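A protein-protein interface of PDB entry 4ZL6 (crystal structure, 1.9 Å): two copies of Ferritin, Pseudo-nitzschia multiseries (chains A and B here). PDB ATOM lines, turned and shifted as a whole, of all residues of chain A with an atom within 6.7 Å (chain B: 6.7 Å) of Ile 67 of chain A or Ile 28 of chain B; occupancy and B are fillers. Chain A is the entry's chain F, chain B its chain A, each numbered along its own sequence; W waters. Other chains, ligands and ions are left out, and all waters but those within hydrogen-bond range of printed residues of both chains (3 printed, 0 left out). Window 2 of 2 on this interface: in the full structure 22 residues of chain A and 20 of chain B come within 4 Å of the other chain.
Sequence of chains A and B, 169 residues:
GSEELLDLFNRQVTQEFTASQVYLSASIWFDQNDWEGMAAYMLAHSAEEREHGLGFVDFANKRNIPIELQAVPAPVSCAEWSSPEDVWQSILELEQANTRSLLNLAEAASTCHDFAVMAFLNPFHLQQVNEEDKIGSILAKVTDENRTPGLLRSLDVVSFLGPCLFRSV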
ATOM      1  N   LEU A   6     -19.957  -5.326  39.362  1.00  0.00           N
ATOM      2  CA  LEU A   6     -19.770  -6.171  38.158  1.00  0.00           C
ATOM      3  C   LEU A   6     -18.877  -5.471  37.094  1.00  0.00           C
ATOM      4  O   LEU A   6     -17.996  -6.056  36.447  1.00  0.00           O
ATOM      5  CB  LEU A   6     -21.139  -6.464  37.510  1.00  0.00           C
ATOM      6  CG  LEU A   6     -22.300  -7.019  38.398  1.00  0.00           C
ATOM      7  CD1 LEU A   6     -23.442  -7.497  37.497  1.00  0.00           C
ATOM      8  CD2 LEU A   6     -21.892  -8.141  39.377  1.00  0.00           C
ATOM      9  N   PHE A   9     -15.291  -5.342  38.370  1.00  0.00           N
ATOM     10  CA  PHE A   9     -14.759  -6.709  38.250  1.00  0.00           C
ATOM     11  C   PHE A   9     -14.319  -6.951  36.824  1.00  0.00           C
ATOM     12  O   PHE A   9     -13.221  -7.414  36.555  1.00  0.00           O
ATOM     13  CB  PHE A   9     -15.787  -7.748  38.748  1.00  0.00           C
ATOM     14  CG  PHE A   9     -15.156  -9.001  39.255  1.00  0.00           C
ATOM     15  CD1 PHE A   9     -14.679  -9.905  38.372  1.00  0.00           C
ATOM     16  CD2 PHE A   9     -14.949  -9.200  40.616  1.00  0.00           C
ATOM     17  CE1 PHE A   9     -14.058 -11.050  38.788  1.00  0.00           C
ATOM     18  CE2 PHE A   9     -14.322 -10.337  41.049  1.00  0.00           C
ATOM     19  CZ  PHE A   9     -13.853 -11.254  40.126  1.00  0.00           C
ATOM     20  N   ASN A  10     -15.176  -6.616  35.850  1.00  0.00           N
ATOM     21  CA  ASN A  10     -14.841  -6.745  34.490  1.00  0.00           C
ATOM     22  C   ASN A  10     -13.610  -5.920  34.095  1.00  0.00           C
ATOM     23  O   ASN A  10     -12.756  -6.363  33.318  1.00  0.00           O
ATOM     24  CB  ASN A  10     -16.104  -6.358  33.696  1.00  0.00           C
ATOM     25  CG  ASN A  10     -16.075  -6.801  32.276  1.00  0.00           C
ATOM     26  OD1 ASN A  10     -16.177  -7.987  31.948  1.00  0.00           O
ATOM     27  ND2 ASN A  10     -15.934  -5.815  31.379  1.00  0.00           N
ATOM     28  N   ARG A  11     -13.523  -4.703  34.614  1.00  0.00           N
ATOM     29  CA  ARG A  11     -12.390  -3.852  34.356  1.00  0.00           C
ATOM     30  C   ARG A  11     -11.070  -4.361  34.969  1.00  0.00           C
ATOM     31  O   ARG A  11     -10.010  -4.048  34.465  1.00  0.00           O
ATOM     32  CB  ARG A  11     -12.666  -2.416  34.899  1.00  0.00           C
ATOM     33  CG  ARG A  11     -13.795  -1.751  34.112  1.00  0.00           C
ATOM     34  CD  ARG A  11     -14.112  -0.303  34.547  1.00  0.00           C
ATOM     35  NE  ARG A  11     -15.280   0.271  33.846  1.00  0.00           N
ATOM     36  CZ  ARG A  11     -15.379   0.556  32.530  1.00  0.00           C
ATOM     37  NH1 ARG A  11     -14.378   0.324  31.683  1.00  0.00           N
ATOM     38  NH2 ARG A  11     -16.498   1.104  32.048  1.00  0.00           N
ATOM     39  N   VAL A  13     -10.084  -7.479  34.971  1.00  0.00           N
ATOM     40  CA  VAL A  13      -9.559  -8.335  33.910  1.00  0.00           C
ATOM     41  C   VAL A  13      -8.778  -7.533  32.851  1.00  0.00           C
ATOM     42  O   VAL A  13      -7.662  -7.848  32.518  1.00  0.00           O
ATOM     43  CB  VAL A  13     -10.664  -9.128  33.209  1.00  0.00           C
ATOM     44  CG1 VAL A  13     -10.077  -9.968  32.112  1.00  0.00           C
ATOM     45  CG2 VAL A  13     -11.329 -10.024  34.213  1.00  0.00           C
ATOM     46  N   PHE A  56      -9.414 -14.014  37.633  1.00  0.00           N
ATOM     47  CA  PHE A  56     -10.604 -13.199  37.754  1.00  0.00           C
ATOM     48  C   PHE A  56     -11.695 -13.708  36.886  1.00  0.00           C
ATOM     49  O   PHE A  56     -12.880 -13.759  37.295  1.00  0.00           O
ATOM     50  CB  PHE A  56     -10.317 -11.721  37.415  1.00  0.00           C
ATOM     51  CG  PHE A  56      -9.752 -10.973  38.591  1.00  0.00           C
ATOM     52  CD1 PHE A  56      -8.467 -11.173  38.972  1.00  0.00           C
ATOM     53  CD2 PHE A  56     -10.566 -10.183  39.403  1.00  0.00           C
ATOM     54  CE1 PHE A  56      -7.919 -10.534  40.104  1.00  0.00           C
ATOM     55  CE2 PHE A  56     -10.047  -9.582  40.553  1.00  0.00           C
ATOM     56  CZ  PHE A  56      -8.707  -9.775  40.903  1.00  0.00           C
ATOM     57  N   VAL A  57     -11.330 -14.046  35.657  1.00  0.00           N
ATOM     58  CA  VAL A  57     -12.316 -14.606  34.749  1.00  0.00           C
ATOM     59  C   VAL A  57     -13.006 -15.848  35.297  1.00  0.00           C
ATOM     60  O   VAL A  57     -14.225 -15.940  35.255  1.00  0.00           O
ATOM     61  CB  VAL A  57     -11.687 -14.909  33.404  1.00  0.00           C
ATOM     62  CG1 VAL A  57     -12.626 -15.777  32.499  1.00  0.00           C
ATOM     63  CG2 VAL A  57     -11.384 -13.586  32.682  1.00  0.00           C
ATOM     64  N   ASP A  58     -12.210 -16.783  35.781  1.00  0.00           N
ATOM     65  CA  ASP A  58     -12.721 -18.048  36.313  1.00  0.00           C
ATOM     66  C   ASP A  58     -13.681 -17.787  37.500  1.00  0.00           C
ATOM     67  O   ASP A  58     -14.777 -18.371  37.572  1.00  0.00           O
ATOM     68  CB  ASP A  58     -11.528 -18.929  36.670  1.00  0.00           C
ATOM     69  CG  ASP A  58     -11.930 -20.271  37.213  1.00  0.00           C
ATOM     70  OD1 ASP A  58     -12.696 -20.937  36.593  1.00  0.00           O
ATOM     71  OD2 ASP A  58     -11.482 -20.618  38.244  1.00  0.00           O
ATOM     72  N   ALA A  60     -15.302 -15.033  38.126  1.00  0.00           N
ATOM     73  CA  ALA A  60     -16.490 -14.423  37.587  1.00  0.00           C
ATOM     74  C   ALA A  60     -17.465 -15.412  37.034  1.00  0.00           C
ATOM     75  O   ALA A  60     -18.692 -15.336  37.256  1.00  0.00           O
ATOM     76  CB  ALA A  60     -16.099 -13.425  36.504  1.00  0.00           C
ATOM     77  N   ASN A  61     -16.948 -16.347  36.279  1.00  0.00           N
ATOM     78  CA  ASN A  61     -17.821 -17.327  35.622  1.00  0.00           C
ATOM     79  C   ASN A  61     -18.596 -18.127  36.707  1.00  0.00           C
ATOM     80  O   ASN A  61     -19.824 -18.340  36.625  1.00  0.00           O
ATOM     81  CB  ASN A  61     -16.977 -18.286  34.796  1.00  0.00           C
ATOM     82  CG  ASN A  61     -16.424 -17.639  33.499  1.00  0.00           C
ATOM     83  OD1 ASN A  61     -16.857 -16.555  33.047  1.00  0.00           O
ATOM     84  ND2 ASN A  61     -15.452 -18.303  32.918  1.00  0.00           N
ATOM     85  N   ILE A  65     -20.834 -13.509  37.268  1.00  0.00           N
ATOM     86  CA  ILE A  65     -20.548 -12.130  36.945  1.00  0.00           C
ATOM     87  C   ILE A  65     -20.217 -12.134  35.441  1.00  0.00           C
ATOM     88  O   ILE A  65     -19.207 -12.752  35.037  1.00  0.00           O
ATOM     89  CB  ILE A  65     -19.370 -11.587  37.753  1.00  0.00           C
ATOM     90  CG1 ILE A  65     -19.666 -11.597  39.285  1.00  0.00           C
ATOM     91  CG2 ILE A  65     -19.099 -10.202  37.244  1.00  0.00           C
ATOM     92  CD1 ILE A  65     -18.430 -11.553  40.151  1.00  0.00           C
ATOM     93  N   PRO A  66     -21.073 -11.530  34.618  1.00  0.00           N
ATOM     94  CA  PRO A  66     -20.863 -11.492  33.203  1.00  0.00           C
ATOM     95  C   PRO A  66     -19.499 -10.865  32.869  1.00  0.00           C
ATOM     96  O   PRO A  66     -19.091  -9.899  33.470  1.00  0.00           O
ATOM     97  CB  PRO A  66     -21.970 -10.560  32.706  1.00  0.00           C
ATOM     98  CG  PRO A  66     -23.003 -10.519  33.794  1.00  0.00           C
ATOM     99  CD  PRO A  66     -22.239 -10.688  35.031  1.00  0.00           C
ATOM    100  N   ILE A  67     -18.733 -11.525  32.042  1.00  0.00           N
ATOM    101  CA  ILE A  67     -17.473 -10.957  31.610  1.00  0.00           C
ATOM    102  C   ILE A  67     -17.672 -10.559  30.148  1.00  0.00           C
ATOM    103  O   ILE A  67     -18.058 -11.370  29.347  1.00  0.00           O
ATOM    104  CB  ILE A  67     -16.337 -11.954  31.728  1.00  0.00           C
ATOM    105  CG1 ILE A  67     -15.964 -12.213  33.167  1.00  0.00           C
ATOM    106  CG2 ILE A  67     -15.126 -11.462  30.941  1.00  0.00           C
ATOM    107  CD1 ILE A  67     -15.469 -10.986  33.921  1.00  0.00           C
ATOM    108  N   GLU A  68     -17.343  -9.335  29.828  1.00  0.00           N
ATOM    109  CA  GLU A  68     -17.197  -8.961  28.467  1.00  0.00           C
ATOM    110  C   GLU A  68     -15.752  -8.477  28.232  1.00  0.00           C
ATOM    111  O   GLU A  68     -15.326  -7.539  28.838  1.00  0.00           O
ATOM    112  CB  GLU A  68     -18.235  -7.888  28.140  1.00  0.00           C
ATOM    113  CG  GLU A  68     -18.972  -8.249  26.859  1.00  0.00           C
ATOM    114  CD  GLU A  68     -19.482  -7.019  26.120  1.00  0.00           C
ATOM    115  OE1 GLU A  68     -19.168  -6.862  24.907  1.00  0.00           O
ATOM    116  OE2 GLU A  68     -20.191  -6.213  26.770  1.00  0.00           O
ATOM    117  N   LEU A  69     -15.005  -9.177  27.389  1.00  0.00           N
ATOM    118  CA  LEU A  69     -13.599  -8.842  27.174  1.00  0.00           C
ATOM    119  C   LEU A  69     -13.449  -7.540  26.406  1.00  0.00           C
ATOM    120  O   LEU A  69     -14.049  -7.378  25.343  1.00  0.00           O
ATOM    121  CB  LEU A  69     -12.897  -9.958  26.429  1.00  0.00           C
ATOM    122  CG  LEU A  69     -12.816 -11.239  27.275  1.00  0.00           C
ATOM    123  CD1 LEU A  69     -12.232 -12.367  26.439  1.00  0.00           C
ATOM    124  CD2 LEU A  69     -12.023 -11.049  28.579  1.00  0.00           C
ATOM    125  N   GLN B  21      -7.476 -14.011  22.490  1.00  0.00           N
ATOM    126  CA  GLN B  21      -8.635 -13.444  23.107  1.00  0.00           C
ATOM    127  C   GLN B  21      -9.906 -14.074  22.637  1.00  0.00           C
ATOM    128  O   GLN B  21     -10.837 -14.261  23.406  1.00  0.00           O
ATOM    129  CB  GLN B  21      -8.707 -11.914  22.876  1.00  0.00           C
ATOM    130  CG  GLN B  21      -7.664 -11.179  23.627  1.00  0.00           C
ATOM    131  CD  GLN B  21      -7.922 -11.157  25.135  1.00  0.00           C
ATOM    132  OE1 GLN B  21      -7.487 -12.042  25.845  1.00  0.00           O
ATOM    133  NE2 GLN B  21      -8.569 -10.127  25.617  1.00  0.00           N
ATOM    134  N   TYR B  23     -10.372 -17.214  21.519  1.00  0.00           N
ATOM    135  CA  TYR B  23     -10.404 -18.474  22.356  1.00  0.00           C
ATOM    136  C   TYR B  23     -10.819 -18.287  23.807  1.00  0.00           C
ATOM    137  O   TYR B  23     -11.655 -19.025  24.317  1.00  0.00           O
ATOM    138  CB  TYR B  23      -9.078 -19.167  22.276  1.00  0.00           C
ATOM    139  CG  TYR B  23      -8.904 -19.975  21.024  1.00  0.00           C
ATOM    140  CD1 TYR B  23      -9.540 -21.208  20.873  1.00  0.00           C
ATOM    141  CD2 TYR B  23      -8.016 -19.591  20.029  1.00  0.00           C
ATOM    142  CE1 TYR B  23      -9.373 -21.992  19.730  1.00  0.00           C
ATOM    143  CE2 TYR B  23      -7.857 -20.348  18.885  1.00  0.00           C
ATOM    144  CZ  TYR B  23      -8.530 -21.549  18.739  1.00  0.00           C
ATOM    145  OH  TYR B  23      -8.359 -22.299  17.615  1.00  0.00           O
ATOM    146  N   LEU B  24     -10.309 -17.239  24.468  1.00  0.00           N
ATOM    147  CA  LEU B  24     -10.754 -16.912  25.785  1.00  0.00           C
ATOM    148  C   LEU B  24     -12.247 -16.612  25.856  1.00  0.00           C
ATOM    149  O   LEU B  24     -12.980 -17.173  26.709  1.00  0.00           O
ATOM    150  CB  LEU B  24      -9.882 -15.782  26.366  1.00  0.00           C
ATOM    151  CG  LEU B  24     -10.269 -15.456  27.809  1.00  0.00           C
ATOM    152  CD1 LEU B  24     -10.179 -16.698  28.726  1.00  0.00           C
ATOM    153  CD2 LEU B  24      -9.402 -14.301  28.232  1.00  0.00           C
ATOM    154  N   SER B  25     -12.761 -15.817  24.902  1.00  0.00           N
ATOM    155  CA  SER B  25     -14.152 -15.554  24.817  1.00  0.00           C
ATOM    156  C   SER B  25     -15.006 -16.803  24.609  1.00  0.00           C
ATOM    157  O   SER B  25     -16.057 -16.900  25.234  1.00  0.00           O
ATOM    158  CB  SER B  25     -14.455 -14.517  23.692  1.00  0.00           C
ATOM    159  OG  SER B  25     -15.820 -14.260  23.675  1.00  0.00           O
ATOM    160  N   ALA B  26     -14.561 -17.734  23.767  1.00  0.00           N
ATOM    161  CA  ALA B  26     -15.218 -19.044  23.574  1.00  0.00           C
ATOM    162  C   ALA B  26     -15.268 -19.838  24.892  1.00  0.00           C
ATOM    163  O   ALA B  26     -16.289 -20.392  25.224  1.00  0.00           O
ATOM    164  CB  ALA B  26     -14.529 -19.835  22.460  1.00  0.00           C
ATOM    165  N   SER B  27     -14.184 -19.814  25.665  1.00  0.00           N
ATOM    166  CA  SER B  27     -14.103 -20.522  26.925  1.00  0.00           C
ATOM    167  C   SER B  27     -15.086 -19.928  27.899  1.00  0.00           C
ATOM    168  O   SER B  27     -15.761 -20.638  28.688  1.00  0.00           O
ATOM    169  CB  SER B  27     -12.686 -20.515  27.507  1.00  0.00           C
ATOM    170  OG  SER B  27     -12.448 -19.383  28.346  1.00  0.00           O
ATOM    171  N   ILE B  28     -15.225 -18.606  27.846  1.00  0.00           N
ATOM    172  CA  ILE B  28     -16.223 -17.957  28.655  1.00  0.00           C
ATOM    173  C   ILE B  28     -17.623 -18.370  28.310  1.00  0.00           C
ATOM    174  O   ILE B  28     -18.430 -18.675  29.236  1.00  0.00           O
ATOM    175  CB  ILE B  28     -16.018 -16.415  28.654  1.00  0.00           C
ATOM    176  CG1 ILE B  28     -14.723 -16.061  29.353  1.00  0.00           C
ATOM    177  CG2 ILE B  28     -17.197 -15.687  29.336  1.00  0.00           C
ATOM    178  CD1 ILE B  28     -14.269 -14.599  29.063  1.00  0.00           C
ATOM    179  N   TRP B  29     -17.977 -18.324  27.033  1.00  0.00           N
ATOM    180  CA  TRP B  29     -19.306 -18.699  26.614  1.00  0.00           C
ATOM    181  C   TRP B  29     -19.574 -20.136  27.070  1.00  0.00           C
ATOM    182  O   TRP B  29     -20.670 -20.472  27.677  1.00  0.00           O
ATOM    183  CB  TRP B  29     -19.446 -18.604  25.095  1.00  0.00           C
ATOM    184  CG  TRP B  29     -20.822 -18.772  24.677  1.00  0.00           C
ATOM    185  CD1 TRP B  29     -21.753 -17.739  24.580  1.00  0.00           C
ATOM    186  CD2 TRP B  29     -21.565 -20.003  24.447  1.00  0.00           C
ATOM    187  NE1 TRP B  29     -23.005 -18.283  24.270  1.00  0.00           N
ATOM    188  CE2 TRP B  29     -22.914 -19.639  24.181  1.00  0.00           C
ATOM    189  CE3 TRP B  29     -21.229 -21.369  24.443  1.00  0.00           C
ATOM    190  CZ2 TRP B  29     -23.911 -20.596  23.871  1.00  0.00           C
ATOM    191  CZ3 TRP B  29     -22.189 -22.286  24.173  1.00  0.00           C
ATOM    192  CH2 TRP B  29     -23.542 -21.897  23.877  1.00  0.00           C
ATOM    193  N   PHE B  30     -18.583 -21.016  26.853  1.00  0.00           N
ATOM    194  CA  PHE B  30     -18.827 -22.404  27.244  1.00  0.00           C
ATOM    195  C   PHE B  30     -19.034 -22.583  28.763  1.00  0.00           C
ATOM    196  O   PHE B  30     -19.926 -23.317  29.214  1.00  0.00           O
ATOM    197  CB  PHE B  30     -17.690 -23.304  26.747  1.00  0.00           C
ATOM    198  CG  PHE B  30     -17.746 -23.597  25.302  1.00  0.00           C
ATOM    199  CD1 PHE B  30     -18.910 -24.064  24.725  1.00  0.00           C
ATOM    200  CD2 PHE B  30     -16.622 -23.488  24.518  1.00  0.00           C
ATOM    201  CE1 PHE B  30     -18.951 -24.396  23.402  1.00  0.00           C
ATOM    202  CE2 PHE B  30     -16.668 -23.767  23.169  1.00  0.00           C
ATOM    203  CZ  PHE B  30     -17.821 -24.223  22.605  1.00  0.00           C
ATOM    204  N   ASP B  31     -18.215 -21.929  29.571  1.00  0.00           N
ATOM    205  CA  ASP B  31     -18.289 -22.073  31.000  1.00  0.00           C
ATOM    206  C   ASP B  31     -19.622 -21.527  31.478  1.00  0.00           C
ATOM    207  O   ASP B  31     -20.293 -22.169  32.292  1.00  0.00           O
ATOM    208  CB  ASP B  31     -17.135 -21.400  31.738  1.00  0.00           C
ATOM    209  CG  ASP B  31     -16.041 -22.362  32.136  1.00  0.00           C
ATOM    210  OD1 ASP B  31     -16.297 -23.566  32.414  1.00  0.00           O
ATOM    211  OD2 ASP B  31     -14.869 -21.929  32.081  1.00  0.00           O
ATOM    212  N   GLN B  32     -20.024 -20.358  30.983  1.00  0.00           N
ATOM    213  CA  GLN B  32     -21.321 -19.782  31.361  1.00  0.00           C
ATOM    214  C   GLN B  32     -22.479 -20.702  31.027  1.00  0.00           C
ATOM    215  O   GLN B  32     -23.542 -20.632  31.663  1.00  0.00           O
ATOM    216  CB  GLN B  32     -21.594 -18.455  30.597  1.00  0.00           C
ATOM    217  CG  GLN B  32     -20.770 -17.271  31.044  1.00  0.00           C
ATOM    218  CD  GLN B  32     -20.883 -16.037  30.114  1.00  0.00           C
ATOM    219  OE1 GLN B  32     -21.280 -16.124  28.922  1.00  0.00           O
ATOM    220  NE2 GLN B  32     -20.416 -14.887  30.633  1.00  0.00           N
ATOM    221  N   ASN B  33     -22.356 -21.483  29.956  1.00  0.00           N
ATOM    222  CA  ASN B  33     -23.434 -22.353  29.529  1.00  0.00           C
ATOM    223  C   ASN B  33     -23.218 -23.827  29.955  1.00  0.00           C
ATOM    224  O   ASN B  33     -23.828 -24.718  29.405  1.00  0.00           O
ATOM    225  CB  ASN B  33     -23.601 -22.167  28.012  1.00  0.00           C
ATOM    226  CG  ASN B  33     -24.223 -20.852  27.713  1.00  0.00           C
ATOM    227  OD1 ASN B  33     -25.411 -20.700  27.957  1.00  0.00           O
ATOM    228  ND2 ASN B  33     -23.409 -19.821  27.425  1.00  0.00           N
ATOM    229  N   ALA B  39     -14.979 -25.746  27.349  1.00  0.00           N
ATOM    230  CA  ALA B  39     -14.380 -24.573  27.959  1.00  0.00           C
ATOM    231  C   ALA B  39     -12.883 -24.759  28.227  1.00  0.00           C
ATOM    232  O   ALA B  39     -12.035 -23.887  27.969  1.00  0.00           O
ATOM    233  CB  ALA B  39     -15.098 -24.165  29.241  1.00  0.00           C
ATOM    234  N   MET B  42     -10.879 -24.697  24.920  1.00  0.00           N
ATOM    235  CA  MET B  42     -10.705 -23.308  24.486  1.00  0.00           C
ATOM    236  C   MET B  42      -9.702 -22.546  25.349  1.00  0.00           C
ATOM    237  O   MET B  42      -8.864 -21.810  24.803  1.00  0.00           O
ATOM    238  CB  MET B  42     -12.053 -22.550  24.455  1.00  0.00           C
ATOM    239  CG  MET B  42     -13.040 -23.054  23.434  1.00  0.00           C
ATOM    240  SD  MET B  42     -12.434 -23.068  21.758  1.00  0.00           S
ATOM    241  CE  MET B  42     -13.743 -23.863  20.885  1.00  0.00           C
ATOM    242  N   TRP B  81     -23.162 -15.911  19.476  1.00  0.00           N
ATOM    243  CA  TRP B  81     -23.212 -17.370  19.730  1.00  0.00           C
ATOM    244  C   TRP B  81     -24.465 -17.770  20.493  1.00  0.00           C
ATOM    245  O   TRP B  81     -24.731 -17.245  21.582  1.00  0.00           O
ATOM    246  CB  TRP B  81     -21.996 -17.764  20.583  1.00  0.00           C
ATOM    247  CG  TRP B  81     -20.699 -17.583  19.836  1.00  0.00           C
ATOM    248  CD1 TRP B  81     -20.519 -17.597  18.473  1.00  0.00           C
ATOM    249  CD2 TRP B  81     -19.390 -17.371  20.414  1.00  0.00           C
ATOM    250  NE1 TRP B  81     -19.195 -17.408  18.185  1.00  0.00           N
ATOM    251  CE2 TRP B  81     -18.494 -17.248  19.362  1.00  0.00           C
ATOM    252  CE3 TRP B  81     -18.919 -17.283  21.721  1.00  0.00           C
ATOM    253  CZ2 TRP B  81     -17.123 -17.020  19.564  1.00  0.00           C
ATOM    254  CZ3 TRP B  81     -17.596 -17.034  21.931  1.00  0.00           C
ATOM    255  CH2 TRP B  81     -16.708 -16.897  20.868  1.00  0.00           C
HETATM  256  O   HOH W   1     -13.357 -19.195  30.922  1.00  0.00           O
HETATM  257  O   HOH W   2     -18.823 -14.823  33.264  1.00  0.00           O
HETATM  258  O   HOH W   3     -20.714 -12.498  29.808  1.00  0.00           O
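The backbone carbonyl oxygen (O) of Leu 24 of chain B sits at hydrogen-bond distance from the side-chain hydroxyl (OG) of Ser 27 of chain B (2.8 Å). The backbone carbonyl oxygen (O) of Val 57 of chain A lies close to the side-chain amide oxygen (OD1) of Asn 61 of chain A.
Among the printed residues, merely in contact across the chains: Asn 61 of chain A with Asp 31 of chain B, Ile 67 of chain A with Ile 28 of chain B, Val 57 of chain A with Ile 28 of chain B, Leu 69 of chain A with Ser 25 of chain B, Asn 61 of chain A with Ile 28 of chain B, Leu 69 of chain A with Gln 21 of chain B and Leu 69 of chain A with Leu 24 of chain B.
Printed residues of chain B within 4 Å of Ile 67 of chain A: Ile 28 (3.8 Å). Of the printed residues of chain A, Ile 28 of chain B touches Val 57 (3.8 Å), Asn 61 (3.8 Å) and Ile 67 (3.8 Å). Printed residues of chain A within 4 Å of Asp 31 of chain B: Asn 61 (3.7 Å). Of the printed residues of chain A, Leu 24 of chain B touches Leu 69. Of the printed residues of chain B, Leu 69 of chain A touches Gln 21, Leu 24 and Ser 25. Of the printed residues of chain A, Ser 25 of chain B touches Leu 69 (3.8 Å). Printed residues of chain B within 4 Å of Asn 61 of chain A: Ile 28 (3.8 Å) and Asp 31 (3.7 Å). Ser 27 of chain B touches none of the printed residues of chain A. Tyr 23 of chain B touches none of the printed residues of chain A. The nearest printed residue of chain B that does not touch Ile 67 of chain A is Gln 32 of chain B (4.02 Å).
Of the 15 printed residues of chain A, 4 touch a printed residue of chain B. Printed residues of chain A that touch a printed residue of chain B: Val 57, Asn 61, Ile 67 and Leu 69. Of the 15 printed residues of chain B, 5 touch a printed residue of chain A. Printed residues of chain B that touch a printed residue of chain A: Gln 21, Leu 24, Ser 25, Ile 28 and Asp 31. Hydrophobic or aromatic side chains of chain B within 4 Å of the printed part of chain A: Leu 24 and Ile 28. Along chain B the printed residues that touch a printed residue of chain A span positions 21 to 31. Among the printed residues, no Asp or Glu carboxylate lies within 4 Å of a Lys or Arg side-chain nitrogen of the other chain.
No position is printed for both chains. Of the 7 pairs that touch across the chains among the printed residues, none has its exchanged pair printed and touching as well.
Water W3 bridges the side-chain amide nitrogen of Gln 32 of chain B (2.5 Å) and the backbone carbonyl oxygen of Ile 67 of chain A (2.9 Å). Water W2 lies within hydrogen-bond range of the side-chain amide oxygen (OD1) of Asn 61 of chain A, the backbone carbonyl oxygen (O) of Ile 65 of chain A and the side-chain amide nitrogen (NE2) of Gln 32 of chain B. Water W1 lies within hydrogen-bond range of OG of Ser 27 of chain B (2.7 Å), ND2 of Asn 61 of chain A (3.0 Å) and OD2 of Asp 31 of chain B (3.3 Å).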
